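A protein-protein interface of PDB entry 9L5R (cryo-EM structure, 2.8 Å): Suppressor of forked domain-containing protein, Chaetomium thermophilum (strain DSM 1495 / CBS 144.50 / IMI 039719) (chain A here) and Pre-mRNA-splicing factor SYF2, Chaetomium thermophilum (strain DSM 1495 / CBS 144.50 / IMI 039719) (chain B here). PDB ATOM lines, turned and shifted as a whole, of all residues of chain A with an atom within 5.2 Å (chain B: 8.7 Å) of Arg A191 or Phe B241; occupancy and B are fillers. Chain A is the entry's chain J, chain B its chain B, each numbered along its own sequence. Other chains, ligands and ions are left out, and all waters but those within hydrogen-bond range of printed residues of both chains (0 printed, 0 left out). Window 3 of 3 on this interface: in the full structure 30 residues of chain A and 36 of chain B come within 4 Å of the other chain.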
ATOM      1  N   ILE A 156       2.061  16.904 -32.794  1.00  0.00           N
ATOM      2  CA  ILE A 156       1.322  17.795 -31.903  1.00  0.00           C
ATOM      3  C   ILE A 156       1.788  17.595 -30.462  1.00  0.00           C
ATOM      4  O   ILE A 156       1.884  18.590 -29.731  1.00  0.00           O
ATOM      5  CB  ILE A 156      -0.202  17.634 -32.073  1.00  0.00           C
ATOM      6  CG1 ILE A 156      -0.602  17.871 -33.526  1.00  0.00           C
ATOM      7  CG2 ILE A 156      -0.952  18.623 -31.223  1.00  0.00           C
ATOM      8  CD1 ILE A 156      -0.055  19.142 -34.119  1.00  0.00           C
ATOM      9  N   PRO A 157       2.105  16.375 -29.991  1.00  0.00           N
ATOM     10  CA  PRO A 157       2.851  16.293 -28.725  1.00  0.00           C
ATOM     11  C   PRO A 157       4.196  16.999 -28.731  1.00  0.00           C
ATOM     12  O   PRO A 157       4.569  17.585 -27.713  1.00  0.00           O
ATOM     13  CB  PRO A 157       2.995  14.785 -28.520  1.00  0.00           C
ATOM     14  CG  PRO A 157       1.772  14.253 -29.076  1.00  0.00           C
ATOM     15  CD  PRO A 157       1.504  15.059 -30.299  1.00  0.00           C
ATOM     16  N   ARG A 160       3.405  20.631 -28.272  1.00  0.00           N
ATOM     17  CA  ARG A 160       3.099  20.853 -26.866  1.00  0.00           C
ATOM     18  C   ARG A 160       4.351  20.843 -26.006  1.00  0.00           C
ATOM     19  O   ARG A 160       4.431  21.586 -25.029  1.00  0.00           O
ATOM     20  CB  ARG A 160       2.128  19.794 -26.379  1.00  0.00           C
ATOM     21  CG  ARG A 160       0.728  20.004 -26.829  1.00  0.00           C
ATOM     22  CD  ARG A 160      -0.194  19.153 -26.011  1.00  0.00           C
ATOM     23  NE  ARG A 160      -1.550  19.156 -26.537  1.00  0.00           N
ATOM     24  CZ  ARG A 160      -2.002  18.291 -27.427  1.00  0.00           C
ATOM     25  NH1 ARG A 160      -1.238  17.326 -27.897  1.00  0.00           N
ATOM     26  NH2 ARG A 160      -3.251  18.399 -27.856  1.00  0.00           N
ATOM     27  N   ASP A 164       5.546  23.951 -23.795  1.00  0.00           N
ATOM     28  CA  ASP A 164       5.702  23.809 -22.354  1.00  0.00           C
ATOM     29  C   ASP A 164       7.043  24.353 -21.877  1.00  0.00           C
ATOM     30  O   ASP A 164       7.118  25.020 -20.836  1.00  0.00           O
ATOM     31  CB  ASP A 164       5.541  22.345 -21.977  1.00  0.00           C
ATOM     32  CG  ASP A 164       4.117  21.983 -21.683  1.00  0.00           C
ATOM     33  OD1 ASP A 164       3.465  22.732 -20.927  1.00  0.00           O
ATOM     34  OD2 ASP A 164       3.647  20.955 -22.205  1.00  0.00           O
ATOM     35  N   TYR A 179      -0.565  29.336 -27.458  1.00  0.00           N
ATOM     36  CA  TYR A 179      -0.710  27.973 -26.963  1.00  0.00           C
ATOM     37  C   TYR A 179      -2.153  27.623 -26.606  1.00  0.00           C
ATOM     38  O   TYR A 179      -2.608  26.493 -26.871  1.00  0.00           O
ATOM     39  CB  TYR A 179       0.314  27.779 -25.851  1.00  0.00           C
ATOM     40  CG  TYR A 179       0.336  26.478 -25.139  1.00  0.00           C
ATOM     41  CD1 TYR A 179       0.499  25.307 -25.835  1.00  0.00           C
ATOM     42  CD2 TYR A 179       0.596  26.448 -23.786  1.00  0.00           C
ATOM     43  CE1 TYR A 179       0.625  24.114 -25.199  1.00  0.00           C
ATOM     44  CE2 TYR A 179       0.759  25.255 -23.127  1.00  0.00           C
ATOM     45  CZ  TYR A 179       0.779  24.091 -23.848  1.00  0.00           C
ATOM     46  OH  TYR A 179       0.939  22.889 -23.225  1.00  0.00           O
ATOM     47  N   GLU A 183      -4.424  24.516 -28.517  1.00  0.00           N
ATOM     48  CA  GLU A 183      -5.340  23.543 -27.928  1.00  0.00           C
ATOM     49  C   GLU A 183      -6.770  23.726 -28.415  1.00  0.00           C
ATOM     50  O   GLU A 183      -7.502  22.744 -28.546  1.00  0.00           O
ATOM     51  CB  GLU A 183      -5.283  23.604 -26.410  1.00  0.00           C
ATOM     52  CG  GLU A 183      -3.895  23.529 -25.876  1.00  0.00           C
ATOM     53  CD  GLU A 183      -3.352  22.130 -25.723  1.00  0.00           C
ATOM     54  OE1 GLU A 183      -3.904  21.181 -26.303  1.00  0.00           O
ATOM     55  OE2 GLU A 183      -2.348  21.979 -25.010  1.00  0.00           O
ATOM     56  N   GLU A 188      -8.950  20.576 -27.495  1.00  0.00           N
ATOM     57  CA  GLU A 188      -8.754  20.284 -26.078  1.00  0.00           C
ATOM     58  C   GLU A 188      -9.053  21.524 -25.256  1.00  0.00           C
ATOM     59  O   GLU A 188      -8.159  22.260 -24.829  1.00  0.00           O
ATOM     60  CB  GLU A 188      -7.355  19.754 -25.825  1.00  0.00           C
ATOM     61  CG  GLU A 188      -7.318  18.264 -25.942  1.00  0.00           C
ATOM     62  CD  GLU A 188      -7.100  17.843 -27.351  1.00  0.00           C
ATOM     63  OE1 GLU A 188      -6.571  18.667 -28.117  1.00  0.00           O
ATOM     64  OE2 GLU A 188      -7.481  16.712 -27.704  1.00  0.00           O
ATOM     65  N   TYR A 189     -10.338  21.723 -24.989  1.00  0.00           N
ATOM     66  CA  TYR A 189     -10.777  22.904 -24.269  1.00  0.00           C
ATOM     67  C   TYR A 189     -10.410  22.842 -22.799  1.00  0.00           C
ATOM     68  O   TYR A 189     -10.176  23.884 -22.184  1.00  0.00           O
ATOM     69  CB  TYR A 189     -12.273  23.073 -24.466  1.00  0.00           C
ATOM     70  CG  TYR A 189     -12.626  23.076 -25.922  1.00  0.00           C
ATOM     71  CD1 TYR A 189     -12.043  23.986 -26.784  1.00  0.00           C
ATOM     72  CD2 TYR A 189     -13.520  22.161 -26.443  1.00  0.00           C
ATOM     73  CE1 TYR A 189     -12.344  23.992 -28.113  1.00  0.00           C
ATOM     74  CE2 TYR A 189     -13.830  22.164 -27.779  1.00  0.00           C
ATOM     75  CZ  TYR A 189     -13.238  23.082 -28.607  1.00  0.00           C
ATOM     76  OH  TYR A 189     -13.540  23.091 -29.942  1.00  0.00           O
ATOM     77  N   GLU A 190     -10.310  21.645 -22.229  1.00  0.00           N
ATOM     78  CA  GLU A 190      -9.844  21.540 -20.854  1.00  0.00           C
ATOM     79  C   GLU A 190      -8.361  21.875 -20.753  1.00  0.00           C
ATOM     80  O   GLU A 190      -7.920  22.504 -19.783  1.00  0.00           O
ATOM     81  CB  GLU A 190     -10.141  20.146 -20.313  1.00  0.00           C
ATOM     82  CG  GLU A 190      -9.559  19.866 -18.946  1.00  0.00           C
ATOM     83  CD  GLU A 190     -10.099  20.791 -17.877  1.00  0.00           C
ATOM     84  OE1 GLU A 190     -11.327  21.012 -17.840  1.00  0.00           O
ATOM     85  OE2 GLU A 190      -9.295  21.299 -17.067  1.00  0.00           O
ATOM     86  N   ARG A 191      -7.581  21.489 -21.761  1.00  0.00           N
ATOM     87  CA  ARG A 191      -6.168  21.844 -21.769  1.00  0.00           C
ATOM     88  C   ARG A 191      -5.983  23.348 -21.925  1.00  0.00           C
ATOM     89  O   ARG A 191      -5.131  23.946 -21.255  1.00  0.00           O
ATOM     90  CB  ARG A 191      -5.451  21.064 -22.867  1.00  0.00           C
ATOM     91  CG  ARG A 191      -5.162  19.636 -22.461  1.00  0.00           C
ATOM     92  CD  ARG A 191      -4.349  18.859 -23.477  1.00  0.00           C
ATOM     93  NE  ARG A 191      -2.937  19.217 -23.472  1.00  0.00           N
ATOM     94  CZ  ARG A 191      -2.060  18.869 -22.538  1.00  0.00           C
ATOM     95  NH1 ARG A 191      -2.409  18.140 -21.494  1.00  0.00           N
ATOM     96  NH2 ARG A 191      -0.802  19.278 -22.649  1.00  0.00           N
ATOM     97  N   ALA A 192      -6.817  23.986 -22.752  1.00  0.00           N
ATOM     98  CA  ALA A 192      -6.808  25.445 -22.851  1.00  0.00           C
ATOM     99  C   ALA A 192      -7.255  26.121 -21.553  1.00  0.00           C
ATOM    100  O   ALA A 192      -6.754  27.200 -21.213  1.00  0.00           O
ATOM    101  CB  ALA A 192      -7.687  25.882 -24.015  1.00  0.00           C
ATOM    102  N   ARG A 193      -8.192  25.510 -20.826  1.00  0.00           N
ATOM    103  CA  ARG A 193      -8.573  25.990 -19.500  1.00  0.00           C
ATOM    104  C   ARG A 193      -7.390  25.971 -18.539  1.00  0.00           C
ATOM    105  O   ARG A 193      -7.183  26.917 -17.762  1.00  0.00           O
ATOM    106  CB  ARG A 193      -9.707  25.113 -18.975  1.00  0.00           C
ATOM    107  CG  ARG A 193     -10.585  25.712 -17.926  1.00  0.00           C
ATOM    108  CD  ARG A 193     -11.823  24.864 -17.754  1.00  0.00           C
ATOM    109  NE  ARG A 193     -12.740  25.043 -18.871  1.00  0.00           N
ATOM    110  CZ  ARG A 193     -13.259  24.053 -19.577  1.00  0.00           C
ATOM    111  NH1 ARG A 193     -13.009  22.792 -19.284  1.00  0.00           N
ATOM    112  NH2 ARG A 193     -14.039  24.336 -20.610  1.00  0.00           N
ATOM    113  N   GLN A 194      -6.603  24.898 -18.578  1.00  0.00           N
ATOM    114  CA  GLN A 194      -5.399  24.823 -17.751  1.00  0.00           C
ATOM    115  C   GLN A 194      -4.392  25.904 -18.132  1.00  0.00           C
ATOM    116  O   GLN A 194      -3.720  26.485 -17.261  1.00  0.00           O
ATOM    117  CB  GLN A 194      -4.777  23.440 -17.877  1.00  0.00           C
ATOM    118  CG  GLN A 194      -5.599  22.344 -17.263  1.00  0.00           C
ATOM    119  CD  GLN A 194      -6.055  22.686 -15.867  1.00  0.00           C
ATOM    120  OE1 GLN A 194      -7.244  22.884 -15.623  1.00  0.00           O
ATOM    121  NE2 GLN A 194      -5.111  22.763 -14.937  1.00  0.00           N
ATOM    122  N   ILE A 195      -4.276  26.190 -19.428  1.00  0.00           N
ATOM    123  CA  ILE A 195      -3.359  27.240 -19.859  1.00  0.00           C
ATOM    124  C   ILE A 195      -3.819  28.609 -19.364  1.00  0.00           C
ATOM    125  O   ILE A 195      -2.990  29.427 -18.979  1.00  0.00           O
ATOM    126  CB  ILE A 195      -3.166  27.228 -21.382  1.00  0.00           C
ATOM    127  CG1 ILE A 195      -2.654  25.879 -21.827  1.00  0.00           C
ATOM    128  CG2 ILE A 195      -2.058  28.172 -21.757  1.00  0.00           C
ATOM    129  CD1 ILE A 195      -2.794  25.680 -23.263  1.00  0.00           C
ATOM    130  N   TYR B 204      -6.230  13.653 -36.499  1.00  0.00           N
ATOM    131  CA  TYR B 204      -5.856  13.883 -35.109  1.00  0.00           C
ATOM    132  C   TYR B 204      -6.514  12.873 -34.190  1.00  0.00           C
ATOM    133  O   TYR B 204      -5.883  12.361 -33.263  1.00  0.00           O
ATOM    134  CB  TYR B 204      -6.241  15.300 -34.687  1.00  0.00           C
ATOM    135  CG  TYR B 204      -5.956  15.602 -33.236  1.00  0.00           C
ATOM    136  CD1 TYR B 204      -4.670  15.859 -32.803  1.00  0.00           C
ATOM    137  CD2 TYR B 204      -6.975  15.622 -32.300  1.00  0.00           C
ATOM    138  CE1 TYR B 204      -4.412  16.128 -31.489  1.00  0.00           C
ATOM    139  CE2 TYR B 204      -6.722  15.890 -30.985  1.00  0.00           C
ATOM    140  CZ  TYR B 204      -5.443  16.141 -30.585  1.00  0.00           C
ATOM    141  OH  TYR B 204      -5.186  16.408 -29.269  1.00  0.00           O
ATOM    142  N   LYS B 208      -4.962   9.950 -31.960  1.00  0.00           N
ATOM    143  CA  LYS B 208      -5.295   9.916 -30.544  1.00  0.00           C
ATOM    144  C   LYS B 208      -5.719   8.524 -30.103  1.00  0.00           C
ATOM    145  O   LYS B 208      -5.279   8.042 -29.059  1.00  0.00           O
ATOM    146  CB  LYS B 208      -6.399  10.926 -30.253  1.00  0.00           C
ATOM    147  CG  LYS B 208      -6.526  11.294 -28.803  1.00  0.00           C
ATOM    148  CD  LYS B 208      -7.384  12.519 -28.634  1.00  0.00           C
ATOM    149  CE  LYS B 208      -7.445  12.926 -27.190  1.00  0.00           C
ATOM    150  NZ  LYS B 208      -8.444  13.984 -26.963  1.00  0.00           N
ATOM    151  N   ALA B 211      -2.714   6.171 -30.200  1.00  0.00           N
ATOM    152  CA  ALA B 211      -1.894   6.416 -29.025  1.00  0.00           C
ATOM    153  C   ALA B 211      -2.565   5.907 -27.763  1.00  0.00           C
ATOM    154  O   ALA B 211      -1.874   5.474 -26.840  1.00  0.00           O
ATOM    155  CB  ALA B 211      -1.585   7.905 -28.900  1.00  0.00           C
ATOM    156  N   ILE B 212      -3.899   5.925 -27.715  1.00  0.00           N
ATOM    157  CA  ILE B 212      -4.613   5.408 -26.550  1.00  0.00           C
ATOM    158  C   ILE B 212      -4.380   3.913 -26.405  1.00  0.00           C
ATOM    159  O   ILE B 212      -4.013   3.432 -25.329  1.00  0.00           O
ATOM    160  CB  ILE B 212      -6.114   5.733 -26.639  1.00  0.00           C
ATOM    161  CG1 ILE B 212      -6.390   7.157 -26.179  1.00  0.00           C
ATOM    162  CG2 ILE B 212      -6.925   4.792 -25.771  1.00  0.00           C
ATOM    163  CD1 ILE B 212      -7.679   7.699 -26.723  1.00  0.00           C
ATOM    164  N   ALA B 215      -0.520   3.246 -25.649  1.00  0.00           N
ATOM    165  CA  ALA B 215      -0.144   3.568 -24.280  1.00  0.00           C
ATOM    166  C   ALA B 215      -0.847   2.668 -23.279  1.00  0.00           C
ATOM    167  O   ALA B 215      -0.305   2.407 -22.200  1.00  0.00           O
ATOM    168  CB  ALA B 215      -0.452   5.032 -23.985  1.00  0.00           C
ATOM    169  N   LEU B 221      -1.361   4.120 -19.700  1.00  0.00           N
ATOM    170  CA  LEU B 221      -2.758   4.529 -19.706  1.00  0.00           C
ATOM    171  C   LEU B 221      -3.588   3.450 -19.030  1.00  0.00           C
ATOM    172  O   LEU B 221      -3.465   2.268 -19.366  1.00  0.00           O
ATOM    173  CB  LEU B 221      -3.274   4.757 -21.129  1.00  0.00           C
ATOM    174  CG  LEU B 221      -3.304   6.177 -21.695  1.00  0.00           C
ATOM    175  CD1 LEU B 221      -3.847   6.152 -23.085  1.00  0.00           C
ATOM    176  CD2 LEU B 221      -4.152   7.082 -20.861  1.00  0.00           C
ATOM    177  N   ALA B 233      -9.850   7.152 -19.819  1.00  0.00           N
ATOM    178  CA  ALA B 233      -8.431   6.850 -19.849  1.00  0.00           C
ATOM    179  C   ALA B 233      -7.705   7.744 -18.860  1.00  0.00           C
ATOM    180  O   ALA B 233      -8.011   8.930 -18.738  1.00  0.00           O
ATOM    181  CB  ALA B 233      -7.866   7.041 -21.253  1.00  0.00           C
ATOM    182  N   VAL B 234      -6.757   7.165 -18.134  1.00  0.00           N
ATOM    183  CA  VAL B 234      -5.966   7.901 -17.160  1.00  0.00           C
ATOM    184  C   VAL B 234      -4.500   7.779 -17.529  1.00  0.00           C
ATOM    185  O   VAL B 234      -3.953   6.670 -17.564  1.00  0.00           O
ATOM    186  CB  VAL B 234      -6.187   7.407 -15.728  1.00  0.00           C
ATOM    187  CG1 VAL B 234      -5.275   8.184 -14.818  1.00  0.00           C
ATOM    188  CG2 VAL B 234      -7.631   7.593 -15.325  1.00  0.00           C
ATOM    189  N   ASP B 235      -3.868   8.915 -17.804  1.00  0.00           N
ATOM    190  CA  ASP B 235      -2.433   8.969 -18.043  1.00  0.00           C
ATOM    191  C   ASP B 235      -1.726   8.882 -16.699  1.00  0.00           C
ATOM    192  O   ASP B 235      -1.866   9.776 -15.860  1.00  0.00           O
ATOM    193  CB  ASP B 235      -2.072  10.253 -18.782  1.00  0.00           C
ATOM    194  CG  ASP B 235      -0.822  10.111 -19.619  1.00  0.00           C
ATOM    195  OD1 ASP B 235      -0.530   8.989 -20.077  1.00  0.00           O
ATOM    196  OD2 ASP B 235      -0.132  11.128 -19.824  1.00  0.00           O
ATOM    197  N   ASP B 237       1.627   8.797 -16.083  1.00  0.00           N
ATOM    198  CA  ASP B 237       2.513   9.942 -16.213  1.00  0.00           C
ATOM    199  C   ASP B 237       1.737  11.081 -16.874  1.00  0.00           C
ATOM    200  O   ASP B 237       0.508  11.060 -16.941  1.00  0.00           O
ATOM    201  CB  ASP B 237       3.778   9.536 -16.965  1.00  0.00           C
ATOM    202  CG  ASP B 237       3.484   8.879 -18.299  1.00  0.00           C
ATOM    203  OD1 ASP B 237       2.298   8.663 -18.621  1.00  0.00           O
ATOM    204  OD2 ASP B 237       4.443   8.564 -19.029  1.00  0.00           O
ATOM    205  N   GLY B 238       2.429  12.111 -17.336  1.00  0.00           N
ATOM    206  CA  GLY B 238       1.738  13.168 -18.043  1.00  0.00           C
ATOM    207  C   GLY B 238       2.172  13.279 -19.486  1.00  0.00           C
ATOM    208  O   GLY B 238       2.058  14.344 -20.098  1.00  0.00           O
ATOM    209  N   THR B 239       2.663  12.180 -20.046  1.00  0.00           N
ATOM    210  CA  THR B 239       3.357  12.204 -21.323  1.00  0.00           C
ATOM    211  C   THR B 239       2.491  11.764 -22.493  1.00  0.00           C
ATOM    212  O   THR B 239       3.021  11.572 -23.590  1.00  0.00           O
ATOM    213  CB  THR B 239       4.609  11.331 -21.259  1.00  0.00           C
ATOM    214  OG1 THR B 239       4.226   9.953 -21.238  1.00  0.00           O
ATOM    215  CG2 THR B 239       5.402  11.643 -20.011  1.00  0.00           C
ATOM    216  N   PHE B 240       1.183  11.579 -22.290  1.00  0.00           N
ATOM    217  CA  PHE B 240       0.315  11.283 -23.424  1.00  0.00           C
ATOM    218  C   PHE B 240       0.252  12.458 -24.385  1.00  0.00           C
ATOM    219  O   PHE B 240       0.502  12.310 -25.586  1.00  0.00           O
ATOM    220  CB  PHE B 240      -1.095  10.919 -22.957  1.00  0.00           C
ATOM    221  CG  PHE B 240      -1.989  10.468 -24.067  1.00  0.00           C
ATOM    222  CD1 PHE B 240      -1.909   9.178 -24.549  1.00  0.00           C
ATOM    223  CD2 PHE B 240      -2.881  11.341 -24.656  1.00  0.00           C
ATOM    224  CE1 PHE B 240      -2.710   8.767 -25.582  1.00  0.00           C
ATOM    225  CE2 PHE B 240      -3.673  10.938 -25.699  1.00  0.00           C
ATOM    226  CZ  PHE B 240      -3.595   9.648 -26.156  1.00  0.00           C
ATOM    227  N   PHE B 241      -0.063  13.637 -23.873  1.00  0.00           N
ATOM    228  CA  PHE B 241      -0.352  14.766 -24.737  1.00  0.00           C
ATOM    229  C   PHE B 241       0.891  15.511 -25.175  1.00  0.00           C
ATOM    230  O   PHE B 241       0.876  16.134 -26.233  1.00  0.00           O
ATOM    231  CB  PHE B 241      -1.308  15.726 -24.037  1.00  0.00           C
ATOM    232  CG  PHE B 241      -2.725  15.268 -24.054  1.00  0.00           C
ATOM    233  CD1 PHE B 241      -3.406  15.151 -25.244  1.00  0.00           C
ATOM    234  CD2 PHE B 241      -3.372  14.945 -22.881  1.00  0.00           C
ATOM    235  CE1 PHE B 241      -4.711  14.731 -25.266  1.00  0.00           C
ATOM    236  CE2 PHE B 241      -4.675  14.521 -22.895  1.00  0.00           C
ATOM    237  CZ  PHE B 241      -5.347  14.413 -24.090  1.00  0.00           C
ATOM    238  N   SER B 242       1.962  15.459 -24.400  1.00  0.00           N
ATOM    239  CA  SER B 242       3.173  16.201 -24.702  1.00  0.00           C
ATOM    240  C   SER B 242       4.380  15.292 -24.561  1.00  0.00           C
ATOM    241  O   SER B 242       4.436  14.461 -23.652  1.00  0.00           O
ATOM    242  CB  SER B 242       3.313  17.411 -23.777  1.00  0.00           C
ATOM    243  OG  SER B 242       4.589  17.995 -23.893  1.00  0.00           O
ATOM    244  N   THR B 243       5.348  15.455 -25.458  1.00  0.00           N
ATOM    245  CA  THR B 243       6.594  14.710 -25.365  1.00  0.00           C
ATOM    246  C   THR B 243       7.588  15.347 -24.404  1.00  0.00           C
ATOM    247  O   THR B 243       8.675  14.799 -24.213  1.00  0.00           O
ATOM    248  CB  THR B 243       7.241  14.551 -26.744  1.00  0.00           C
ATOM    249  OG1 THR B 243       7.402  15.832 -27.357  1.00  0.00           O
ATOM    250  CG2 THR B 243       6.403  13.669 -27.635  1.00  0.00           C
ATOM    251  N   ALA B 244       7.257  16.488 -23.813  1.00  0.00           N
ATOM    252  CA  ALA B 244       7.985  16.943 -22.642  1.00  0.00           C
ATOM    253  C   ALA B 244       7.690  15.994 -21.495  1.00  0.00           C
ATOM    254  O   ALA B 244       6.552  15.537 -21.336  1.00  0.00           O
ATOM    255  CB  ALA B 244       7.589  18.368 -22.276  1.00  0.00           C
ATOM    256  N   ALA B 246       8.681  13.048 -21.596  1.00  0.00           N
ATOM    257  CA  ALA B 246       8.755  11.730 -22.204  1.00  0.00           C
ATOM    258  C   ALA B 246      10.208  11.408 -22.512  1.00  0.00           C
ATOM    259  O   ALA B 246      10.895  12.195 -23.166  1.00  0.00           O
ATOM    260  CB  ALA B 246       7.917  11.671 -23.480  1.00  0.00           C
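NE of Arg A160 is in salt-bridge range of OE1 of Glu A183. The backbone NH of Ala B244 sits at hydrogen-bond distance from the side-chain hydroxyl of Ser B242 (3.1 Å). N of Glu A188 sits at hydrogen-bond distance from O of Glu A183, at 2.8 Å. The side-chain carboxylate of Asp A164 is in hydrogen-bond range of the side-chain hydroxyl of Tyr A179 (3.4 Å). The guanidinium group (NH2) of Arg A160 lies within salt-bridge range of the side-chain carboxylate (OE1) of Glu A188. The side-chain carboxylate (OE2) of Glu A183 lies within salt-bridge range of the guanidinium group (NE) of Arg A191 (3.2 Å).
Among the printed residues, pairs that only touch across the chains: Pro A157 with Phe B241, Asp A164 with Ser B242, Arg A160 with Ser B242, Arg A191 with Phe B241 and Pro A157 with Ser B242.
The side-chain hydroxyl (OH) of Tyr B204 lies within hydrogen-bond range of the side-chain carboxylate (OE2) of Glu A188 (2.8 Å). NZ of Lys B208 lies within salt-bridge range of OE2 of Glu A188. O of Pro A157 is in hydrogen-bond range of N of Thr B243 (3.2 Å). The side-chain hydroxyl (OH) of Tyr B204 is in hydrogen-bond range of the guanidinium group (NH2) of Arg A160, 3.1 Å away. O of Phe B241 lies within hydrogen-bond range of NH1 of Arg A160 (2.9 Å).
Printed residues of chain B within 4 Å of Arg A160: Tyr B204, Phe B241 and Ser B242. Printed residues of chain B within 4 Å of Asp A164: Ser B242 (3.5 Å). Printed residues of chain B within 4 Å of Glu A188: Tyr B204 (2.8 Å) and Lys B208 (3.0 Å). Arg A191 touches one residue of chain B. No residue of chain B comes within 4 Å of Ala A192. Of the printed residues of chain A, Lys B208 touches Glu A188 (3.0 Å). Of the printed residues of chain A, Thr B243 touches Pro A157 (3.2 Å). The nearest residue of chain B that does not touch Arg A191 is Ser B242 (4.7 Å). The nearest printed residue of chain A that does not touch Tyr B204 is Ile A156 (4.3 Å).
Of the 14 printed residues of chain A, 5 touch a printed residue of chain B. Printed residues of chain A that touch a printed residue of chain B: Pro A157, Arg A160, Asp A164, Glu A188 and Arg A191. Along chain A the printed residues that touch a printed residue of chain B span positions 157 to 191. Hydrophobic or aromatic side chains of chain B that line the printed part of chain A: Tyr B204 and Phe B241. Among the printed residues, Asp or Glu carboxylates within 4 Å of a Lys or Arg side-chain nitrogen of the other chain: Glu A188 with Lys B208.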
